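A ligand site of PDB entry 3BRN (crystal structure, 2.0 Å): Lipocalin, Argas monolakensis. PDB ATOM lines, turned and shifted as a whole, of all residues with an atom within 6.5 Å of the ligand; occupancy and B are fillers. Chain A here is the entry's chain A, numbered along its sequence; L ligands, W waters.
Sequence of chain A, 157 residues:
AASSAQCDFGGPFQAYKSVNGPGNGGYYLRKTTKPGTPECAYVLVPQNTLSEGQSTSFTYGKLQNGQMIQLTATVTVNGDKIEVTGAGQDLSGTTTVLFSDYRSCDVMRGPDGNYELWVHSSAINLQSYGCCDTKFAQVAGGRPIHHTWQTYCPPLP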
ATOM      1  N   ALA A  15     -15.882 -16.091 -17.875  1.00  0.00           N
ATOM      2  CA  ALA A  15     -14.988 -15.919 -16.755  1.00  0.00           C
ATOM      3  C   ALA A  15     -13.491 -15.854 -17.047  1.00  0.00           C
ATOM      4  O   ALA A  15     -12.790 -15.030 -16.482  1.00  0.00           O
ATOM      5  CB  ALA A  15     -15.294 -16.948 -15.667  1.00  0.00           C
ATOM      6  N   LYS A  17     -12.034 -14.778 -19.693  1.00  0.00           N
ATOM      7  CA  LYS A  17     -11.816 -13.454 -20.281  1.00  0.00           C
ATOM      8  C   LYS A  17     -11.914 -12.320 -19.263  1.00  0.00           C
ATOM      9  O   LYS A  17     -11.190 -11.339 -19.333  1.00  0.00           O
ATOM     10  CB  LYS A  17     -12.758 -13.207 -21.452  1.00  0.00           C
ATOM     11  CG  LYS A  17     -12.357 -13.903 -22.735  1.00  0.00           C
ATOM     12  CD  LYS A  17     -13.562 -14.297 -23.549  1.00  0.00           C
ATOM     13  CE  LYS A  17     -13.181 -14.714 -24.952  1.00  0.00           C
ATOM     14  NZ  LYS A  17     -13.157 -13.539 -25.863  1.00  0.00           N
ATOM     15  N   SER A  18     -12.865 -12.432 -18.329  1.00  0.00           N
ATOM     16  CA  SER A  18     -12.964 -11.466 -17.256  1.00  0.00           C
ATOM     17  C   SER A  18     -11.697 -11.478 -16.380  1.00  0.00           C
ATOM     18  O   SER A  18     -11.142 -10.434 -16.030  1.00  0.00           O
ATOM     19  CB  SER A  18     -14.201 -11.745 -16.392  1.00  0.00           C
ATOM     20  OG  SER A  18     -14.188 -10.909 -15.244  1.00  0.00           O
ATOM     21  N   VAL A  19     -11.283 -12.661 -15.965  1.00  0.00           N
ATOM     22  CA  VAL A  19     -10.141 -12.807 -15.056  1.00  0.00           C
ATOM     23  C   VAL A  19      -8.821 -12.395 -15.737  1.00  0.00           C
ATOM     24  O   VAL A  19      -7.938 -11.816 -15.094  1.00  0.00           O
ATOM     25  CB  VAL A  19     -10.036 -14.257 -14.533  1.00  0.00           C
ATOM     26  CG1 VAL A  19      -8.735 -14.472 -13.762  1.00  0.00           C
ATOM     27  CG2 VAL A  19     -11.274 -14.607 -13.707  1.00  0.00           C
ATOM     28  N   ASN A  20      -8.651 -12.652 -17.013  1.00  0.00           N
ATOM     29  CA  ASN A  20      -7.515 -12.123 -17.728  1.00  0.00           C
ATOM     30  C   ASN A  20      -7.563 -10.654 -17.975  1.00  0.00           C
ATOM     31  O   ASN A  20      -6.570 -10.021 -17.985  1.00  0.00           O
ATOM     32  CB  ASN A  20      -7.377 -12.803 -19.065  1.00  0.00           C
ATOM     33  CG  ASN A  20      -6.942 -14.198 -18.963  1.00  0.00           C
ATOM     34  OD1 ASN A  20      -6.242 -14.586 -18.083  1.00  0.00           O
ATOM     35  ND2 ASN A  20      -7.337 -14.965 -19.913  1.00  0.00           N
ATOM     36  N   GLY A  21      -8.736 -10.131 -18.240  1.00  0.00           N
ATOM     37  CA  GLY A  21      -8.915  -8.706 -18.443  1.00  0.00           C
ATOM     38  C   GLY A  21      -8.063  -8.161 -19.573  1.00  0.00           C
ATOM     39  O   GLY A  21      -7.797  -8.872 -20.544  1.00  0.00           O
ATOM     40  N   TYR A  27      -7.357  -5.474 -10.541  1.00  0.00           N
ATOM     41  CA  TYR A  27      -8.680  -4.909 -10.322  1.00  0.00           C
ATOM     42  C   TYR A  27      -8.899  -4.570  -8.841  1.00  0.00           C
ATOM     43  O   TYR A  27      -8.632  -5.397  -7.964  1.00  0.00           O
ATOM     44  CB  TYR A  27      -9.768  -5.889 -10.792  1.00  0.00           C
ATOM     45  CG  TYR A  27      -9.897  -5.987 -12.301  1.00  0.00           C
ATOM     46  CD1 TYR A  27     -10.945  -5.380 -12.975  1.00  0.00           C
ATOM     47  CD2 TYR A  27      -9.024  -6.791 -13.027  1.00  0.00           C
ATOM     48  CE1 TYR A  27     -11.063  -5.485 -14.364  1.00  0.00           C
ATOM     49  CE2 TYR A  27      -9.135  -6.916 -14.389  1.00  0.00           C
ATOM     50  CZ  TYR A  27     -10.164  -6.288 -15.052  1.00  0.00           C
ATOM     51  OH  TYR A  27     -10.209  -6.375 -16.417  1.00  0.00           O
ATOM     52  N   VAL A  43      -7.440  -7.747  -6.634  1.00  0.00           N
ATOM     53  CA  VAL A  43      -6.862  -8.963  -7.162  1.00  0.00           C
ATOM     54  C   VAL A  43      -5.915  -8.531  -8.261  1.00  0.00           C
ATOM     55  O   VAL A  43      -6.094  -7.448  -8.824  1.00  0.00           O
ATOM     56  CB  VAL A  43      -7.934  -9.915  -7.795  1.00  0.00           C
ATOM     57  CG1 VAL A  43      -8.852 -10.468  -6.728  1.00  0.00           C
ATOM     58  CG2 VAL A  43      -8.736  -9.202  -8.905  1.00  0.00           C
ATOM     59  N   LEU A  44      -4.870  -9.322  -8.514  1.00  0.00           N
ATOM     60  CA  LEU A  44      -4.024  -9.121  -9.680  1.00  0.00           C
ATOM     61  C   LEU A  44      -4.433 -10.145 -10.728  1.00  0.00           C
ATOM     62  O   LEU A  44      -4.764 -11.287 -10.370  1.00  0.00           O
ATOM     63  CB  LEU A  44      -2.541  -9.335  -9.316  1.00  0.00           C
ATOM     64  CG  LEU A  44      -1.851  -8.280  -8.446  1.00  0.00           C
ATOM     65  CD1 LEU A  44      -0.339  -8.563  -8.373  1.00  0.00           C
ATOM     66  CD2 LEU A  44      -2.081  -6.895  -9.013  1.00  0.00           C
ATOM     67  N   VAL A  45      -4.397  -9.773 -12.003  1.00  0.00           N
ATOM     68  CA  VAL A  45      -4.628 -10.753 -13.073  1.00  0.00           C
ATOM     69  C   VAL A  45      -3.540 -11.847 -13.007  1.00  0.00           C
ATOM     70  O   VAL A  45      -2.417 -11.570 -12.560  1.00  0.00           O
ATOM     71  CB  VAL A  45      -4.682 -10.087 -14.482  1.00  0.00           C
ATOM     72  CG1 VAL A  45      -5.559  -8.848 -14.458  1.00  0.00           C
ATOM     73  CG2 VAL A  45      -3.272  -9.783 -15.006  1.00  0.00           C
ATOM     74  N   PRO A  46      -3.911 -13.116 -13.244  1.00  0.00           N
ATOM     75  CA  PRO A  46      -2.949 -14.203 -13.039  1.00  0.00           C
ATOM     76  C   PRO A  46      -1.705 -13.993 -13.889  1.00  0.00           C
ATOM     77  O   PRO A  46      -1.761 -13.287 -14.904  1.00  0.00           O
ATOM     78  CB  PRO A  46      -3.716 -15.451 -13.503  1.00  0.00           C
ATOM     79  CG  PRO A  46      -5.135 -15.070 -13.361  1.00  0.00           C
ATOM     80  CD  PRO A  46      -5.202 -13.627 -13.726  1.00  0.00           C
ATOM     81  N   PHE A  58      -3.414 -16.869  -8.187  1.00  0.00           N
ATOM     82  CA  PHE A  58      -3.499 -15.440  -8.384  1.00  0.00           C
ATOM     83  C   PHE A  58      -3.249 -14.749  -7.062  1.00  0.00           C
ATOM     84  O   PHE A  58      -3.369 -15.364  -6.005  1.00  0.00           O
ATOM     85  CB  PHE A  58      -4.863 -15.020  -8.951  1.00  0.00           C
ATOM     86  CG  PHE A  58      -5.996 -15.125  -7.962  1.00  0.00           C
ATOM     87  CD1 PHE A  58      -6.534 -16.359  -7.640  1.00  0.00           C
ATOM     88  CD2 PHE A  58      -6.507 -13.992  -7.361  1.00  0.00           C
ATOM     89  CE1 PHE A  58      -7.513 -16.464  -6.689  1.00  0.00           C
ATOM     90  CE2 PHE A  58      -7.505 -14.081  -6.424  1.00  0.00           C
ATOM     91  CZ  PHE A  58      -8.035 -15.320  -6.104  1.00  0.00           C
ATOM     92  N   THR A  59      -2.750 -13.522  -7.149  1.00  0.00           N
ATOM     93  CA  THR A  59      -2.473 -12.713  -5.960  1.00  0.00           C
ATOM     94  C   THR A  59      -3.668 -11.812  -5.666  1.00  0.00           C
ATOM     95  O   THR A  59      -4.339 -11.330  -6.582  1.00  0.00           O
ATOM     96  CB  THR A  59      -1.219 -11.857  -6.163  1.00  0.00           C
ATOM     97  OG1 THR A  59      -0.108 -12.700  -6.523  1.00  0.00           O
ATOM     98  CG2 THR A  59      -0.872 -11.059  -4.896  1.00  0.00           C
ATOM     99  N   VAL A  75      -7.820 -19.895  -8.486  1.00  0.00           N
ATOM    100  CA  VAL A  75      -9.043 -19.530  -9.195  1.00  0.00           C
ATOM    101  C   VAL A  75      -9.218 -20.478 -10.392  1.00  0.00           C
ATOM    102  O   VAL A  75      -8.250 -20.765 -11.109  1.00  0.00           O
ATOM    103  CB  VAL A  75      -8.964 -18.072  -9.686  1.00  0.00           C
ATOM    104  CG1 VAL A  75      -7.893 -17.947 -10.785  1.00  0.00           C
ATOM    105  CG2 VAL A  75     -10.351 -17.580 -10.170  1.00  0.00           C
ATOM    106  N   ILE A  82     -16.345 -17.808 -11.659  1.00  0.00           N
ATOM    107  CA  ILE A  82     -14.999 -17.685 -11.098  1.00  0.00           C
ATOM    108  C   ILE A  82     -15.017 -18.343  -9.726  1.00  0.00           C
ATOM    109  O   ILE A  82     -15.734 -17.900  -8.831  1.00  0.00           O
ATOM    110  CB  ILE A  82     -14.580 -16.195 -10.924  1.00  0.00           C
ATOM    111  CG1 ILE A  82     -14.495 -15.500 -12.289  1.00  0.00           C
ATOM    112  CG2 ILE A  82     -13.217 -16.077 -10.191  1.00  0.00           C
ATOM    113  CD1 ILE A  82     -14.365 -13.985 -12.193  1.00  0.00           C
ATOM    114  N   VAL A  84     -13.143 -19.609  -6.456  1.00  0.00           N
ATOM    115  CA  VAL A  84     -11.938 -19.310  -5.705  1.00  0.00           C
ATOM    116  C   VAL A  84     -11.815 -20.271  -4.521  1.00  0.00           C
ATOM    117  O   VAL A  84     -12.817 -20.641  -3.897  1.00  0.00           O
ATOM    118  CB  VAL A  84     -11.910 -17.845  -5.206  1.00  0.00           C
ATOM    119  CG1 VAL A  84     -10.818 -17.664  -4.161  1.00  0.00           C
ATOM    120  CG2 VAL A  84     -11.694 -16.892  -6.358  1.00  0.00           C
ATOM    121  N   LEU A  91     -12.999 -14.042  -0.202  1.00  0.00           N
ATOM    122  CA  LEU A  91     -13.007 -14.237  -1.641  1.00  0.00           C
ATOM    123  C   LEU A  91     -13.311 -15.678  -2.064  1.00  0.00           C
ATOM    124  O   LEU A  91     -13.678 -15.918  -3.221  1.00  0.00           O
ATOM    125  CB  LEU A  91     -11.683 -13.763  -2.214  1.00  0.00           C
ATOM    126  CG  LEU A  91     -11.606 -13.256  -3.653  1.00  0.00           C
ATOM    127  CD1 LEU A  91     -12.667 -12.189  -3.917  1.00  0.00           C
ATOM    128  CD2 LEU A  91     -10.195 -12.716  -3.893  1.00  0.00           C
ATOM    129  N   THR A  95     -17.867 -16.810  -7.566  1.00  0.00           N
ATOM    130  CA  THR A  95     -18.216 -15.480  -8.063  1.00  0.00           C
ATOM    131  C   THR A  95     -18.759 -15.624  -9.488  1.00  0.00           C
ATOM    132  O   THR A  95     -18.169 -16.331 -10.308  1.00  0.00           O
ATOM    133  CB  THR A  95     -16.967 -14.600  -8.071  1.00  0.00           C
ATOM    134  OG1 THR A  95     -16.586 -14.288  -6.724  1.00  0.00           O
ATOM    135  CG2 THR A  95     -17.202 -13.328  -8.862  1.00  0.00           C
ATOM    136  N   SER A 100     -19.140  -7.842 -18.138  1.00  0.00           N
ATOM    137  CA  SER A 100     -17.741  -7.451 -18.171  1.00  0.00           C
ATOM    138  C   SER A 100     -17.437  -6.919 -19.561  1.00  0.00           C
ATOM    139  O   SER A 100     -18.132  -7.271 -20.508  1.00  0.00           O
ATOM    140  CB  SER A 100     -16.849  -8.655 -17.888  1.00  0.00           C
ATOM    141  OG  SER A 100     -15.492  -8.268 -17.811  1.00  0.00           O
ATOM    142  N   CYS A 105     -13.506  -3.150 -16.434  1.00  0.00           N
ATOM    143  CA  CYS A 105     -14.429  -3.314 -15.308  1.00  0.00           C
ATOM    144  C   CYS A 105     -15.290  -4.577 -15.415  1.00  0.00           C
ATOM    145  O   CYS A 105     -15.522  -5.089 -16.501  1.00  0.00           O
ATOM    146  CB  CYS A 105     -15.310  -2.071 -15.157  1.00  0.00           C
ATOM    147  SG  CYS A 105     -16.406  -1.799 -16.567  1.00  0.00           S
ATOM    148  N   ASP A 106     -15.768  -5.065 -14.286  1.00  0.00           N
ATOM    149  CA  ASP A 106     -16.644  -6.208 -14.206  1.00  0.00           C
ATOM    150  C   ASP A 106     -17.761  -5.908 -13.241  1.00  0.00           C
ATOM    151  O   ASP A 106     -17.547  -5.220 -12.278  1.00  0.00           O
ATOM    152  CB  ASP A 106     -15.945  -7.407 -13.638  1.00  0.00           C
ATOM    153  CG  ASP A 106     -14.624  -7.682 -14.248  1.00  0.00           C
ATOM    154  OD1 ASP A 106     -14.560  -8.007 -15.427  1.00  0.00           O
ATOM    155  OD2 ASP A 106     -13.661  -7.650 -13.526  1.00  0.00           O
ATOM    156  N   MET A 108     -20.088  -8.350 -10.735  1.00  0.00           N
ATOM    157  CA  MET A 108     -20.151  -9.717 -10.278  1.00  0.00           C
ATOM    158  C   MET A 108     -21.312  -9.887  -9.309  1.00  0.00           C
ATOM    159  O   MET A 108     -21.691  -8.938  -8.607  1.00  0.00           O
ATOM    160  CB  MET A 108     -18.870 -10.057  -9.490  1.00  0.00           C
ATOM    161  CG  MET A 108     -17.549  -9.806 -10.198  1.00  0.00           C
ATOM    162  SD  MET A 108     -17.390 -10.670 -11.757  1.00  0.00           S
ATOM    163  CE  MET A 108     -15.603 -10.607 -11.946  1.00  0.00           C
ATOM    164  N   GLU A 116     -21.076  -6.630  -6.831  1.00  0.00           N
ATOM    165  CA  GLU A 116     -19.737  -6.065  -6.772  1.00  0.00           C
ATOM    166  C   GLU A 116     -19.381  -5.379  -8.073  1.00  0.00           C
ATOM    167  O   GLU A 116     -19.606  -5.935  -9.161  1.00  0.00           O
ATOM    168  CB  GLU A 116     -18.708  -7.169  -6.522  1.00  0.00           C
ATOM    169  CG  GLU A 116     -18.894  -7.874  -5.172  1.00  0.00           C
ATOM    170  CD  GLU A 116     -17.910  -9.004  -4.961  1.00  0.00           C
ATOM    171  OE1 GLU A 116     -17.238  -9.419  -5.936  1.00  0.00           O
ATOM    172  OE2 GLU A 116     -17.865  -9.548  -3.834  1.00  0.00           O
ATOM    173  N   TRP A 118     -15.918  -4.279  -9.893  1.00  0.00           N
ATOM    174  CA  TRP A 118     -14.482  -4.333  -9.889  1.00  0.00           C
ATOM    175  C   TRP A 118     -13.949  -3.485 -11.017  1.00  0.00           C
ATOM    176  O   TRP A 118     -14.483  -3.508 -12.073  1.00  0.00           O
ATOM    177  CB  TRP A 118     -14.000  -5.757 -10.000  1.00  0.00           C
ATOM    178  CG  TRP A 118     -14.298  -6.643  -8.891  1.00  0.00           C
ATOM    179  CD1 TRP A 118     -15.455  -7.237  -8.656  1.00  0.00           C
ATOM    180  CD2 TRP A 118     -13.417  -7.044  -7.869  1.00  0.00           C
ATOM    181  NE1 TRP A 118     -15.384  -8.000  -7.553  1.00  0.00           N
ATOM    182  CE2 TRP A 118     -14.128  -7.893  -7.032  1.00  0.00           C
ATOM    183  CE3 TRP A 118     -12.104  -6.759  -7.557  1.00  0.00           C
ATOM    184  CZ2 TRP A 118     -13.558  -8.493  -5.938  1.00  0.00           C
ATOM    185  CZ3 TRP A 118     -11.555  -7.354  -6.459  1.00  0.00           C
ATOM    186  CH2 TRP A 118     -12.267  -8.199  -5.673  1.00  0.00           C
HETATM  187  O1  LIG L   1      -8.923 -13.803  -9.940  1.00  0.00           O
HETATM  188  C1  LIG L   1     -10.121 -13.263  -9.531  1.00  0.00           C
HETATM  189  C2  LIG L   1     -10.804 -13.914  -8.507  1.00  0.00           C
HETATM  190  C3  LIG L   1     -11.965 -13.351  -7.964  1.00  0.00           C
HETATM  191  C4  LIG L   1     -12.437 -12.184  -8.549  1.00  0.00           C
HETATM  192  N1  LIG L   1     -13.517 -11.398  -8.353  1.00  0.00           N
HETATM  193  C5  LIG L   1     -13.465 -10.338  -9.201  1.00  0.00           C
HETATM  194  C6  LIG L   1     -12.323 -10.471  -9.997  1.00  0.00           C
HETATM  195  C7  LIG L   1     -11.695 -11.640  -9.586  1.00  0.00           C
HETATM  196  C8  LIG L   1     -10.593 -12.165 -10.048  1.00  0.00           C
HETATM  197  C9  LIG L   1     -11.904  -9.525 -11.103  1.00  0.00           C
HETATM  198  C10 LIG L   1     -11.988 -10.237 -12.460  1.00  0.00           C
HETATM  199  N2  LIG L   1     -11.417  -9.351 -13.482  1.00  0.00           N
HETATM  200  O   HOH W   1     -15.629 -11.788  -6.110  1.00  0.00           O
HETATM  201  O   HOH W   2      -8.772 -10.454 -12.748  1.00  0.00           O
HETATM  202  O   HOH W   3      -7.276 -12.154 -11.155  1.00  0.00           O
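The backbone carbonyl oxygen (O) of Ser 18 sits at hydrogen-bond distance from a nitrogen (N2) of the ligand (2.8 Å).
The side-chain carboxylate (OD2) of Asp 106 lies within salt-bridge range of a nitrogen (N2) of the ligand (2.8 Å).
The side-chain hydroxyl (OG) of Ser 18 sits at hydrogen-bond distance from the side-chain carboxylate (OD1) of Asp 106, at 2.9 Å.
N of Asp 106 sits at hydrogen-bond distance from O of Trp 118, at 3.0 Å.
The side-chain carboxylate (OD1) of Asp 106 lies within hydrogen-bond range of the side-chain hydroxyl (OG) of Ser 100 (2.6 Å).
The indole nitrogen (NE1) of Trp 118 sits at hydrogen-bond distance from the side-chain carboxylate (OE1) of Glu 116 (2.8 Å).
The backbone NH of Tyr 27 is in hydrogen-bond range of the backbone carbonyl oxygen of Val 43 (2.9 Å).
O of Glu 116 sits at hydrogen-bond distance from N of Met 108 (2.9 Å).
The backbone carbonyl oxygen (O) of Thr 95 sits at hydrogen-bond distance from the backbone NH (N) of Ile 82 (2.7 Å).
Residues that only touch the ligand: Val 19, Tyr 27, Val 43, Phe 58, Ile 82, Val 84, Met 108 and Trp 118.
Hydrophobic or aromatic side chains that line the ligand: Val 19, Tyr 27, Val 43, Phe 58, Ile 82, Val 84, Met 108 and Trp 118.
The nearest printed residue that does not touch the ligand is Val 75 (4.04 Å).
Water W3 lies within hydrogen-bond range of an oxygen (O1) of the ligand (2.6 Å) and the backbone carbonyl oxygen of Leu 44 (2.8 Å).
Water W2 bridges O of Val 19 (2.8 Å) and N2 of the ligand (3.0 Å).
Water W1 lies within hydrogen-bond range of the side-chain hydroxyl of Thr 95, the side-chain carboxylate of Glu 116 and a nitrogen (N1) of the ligand.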
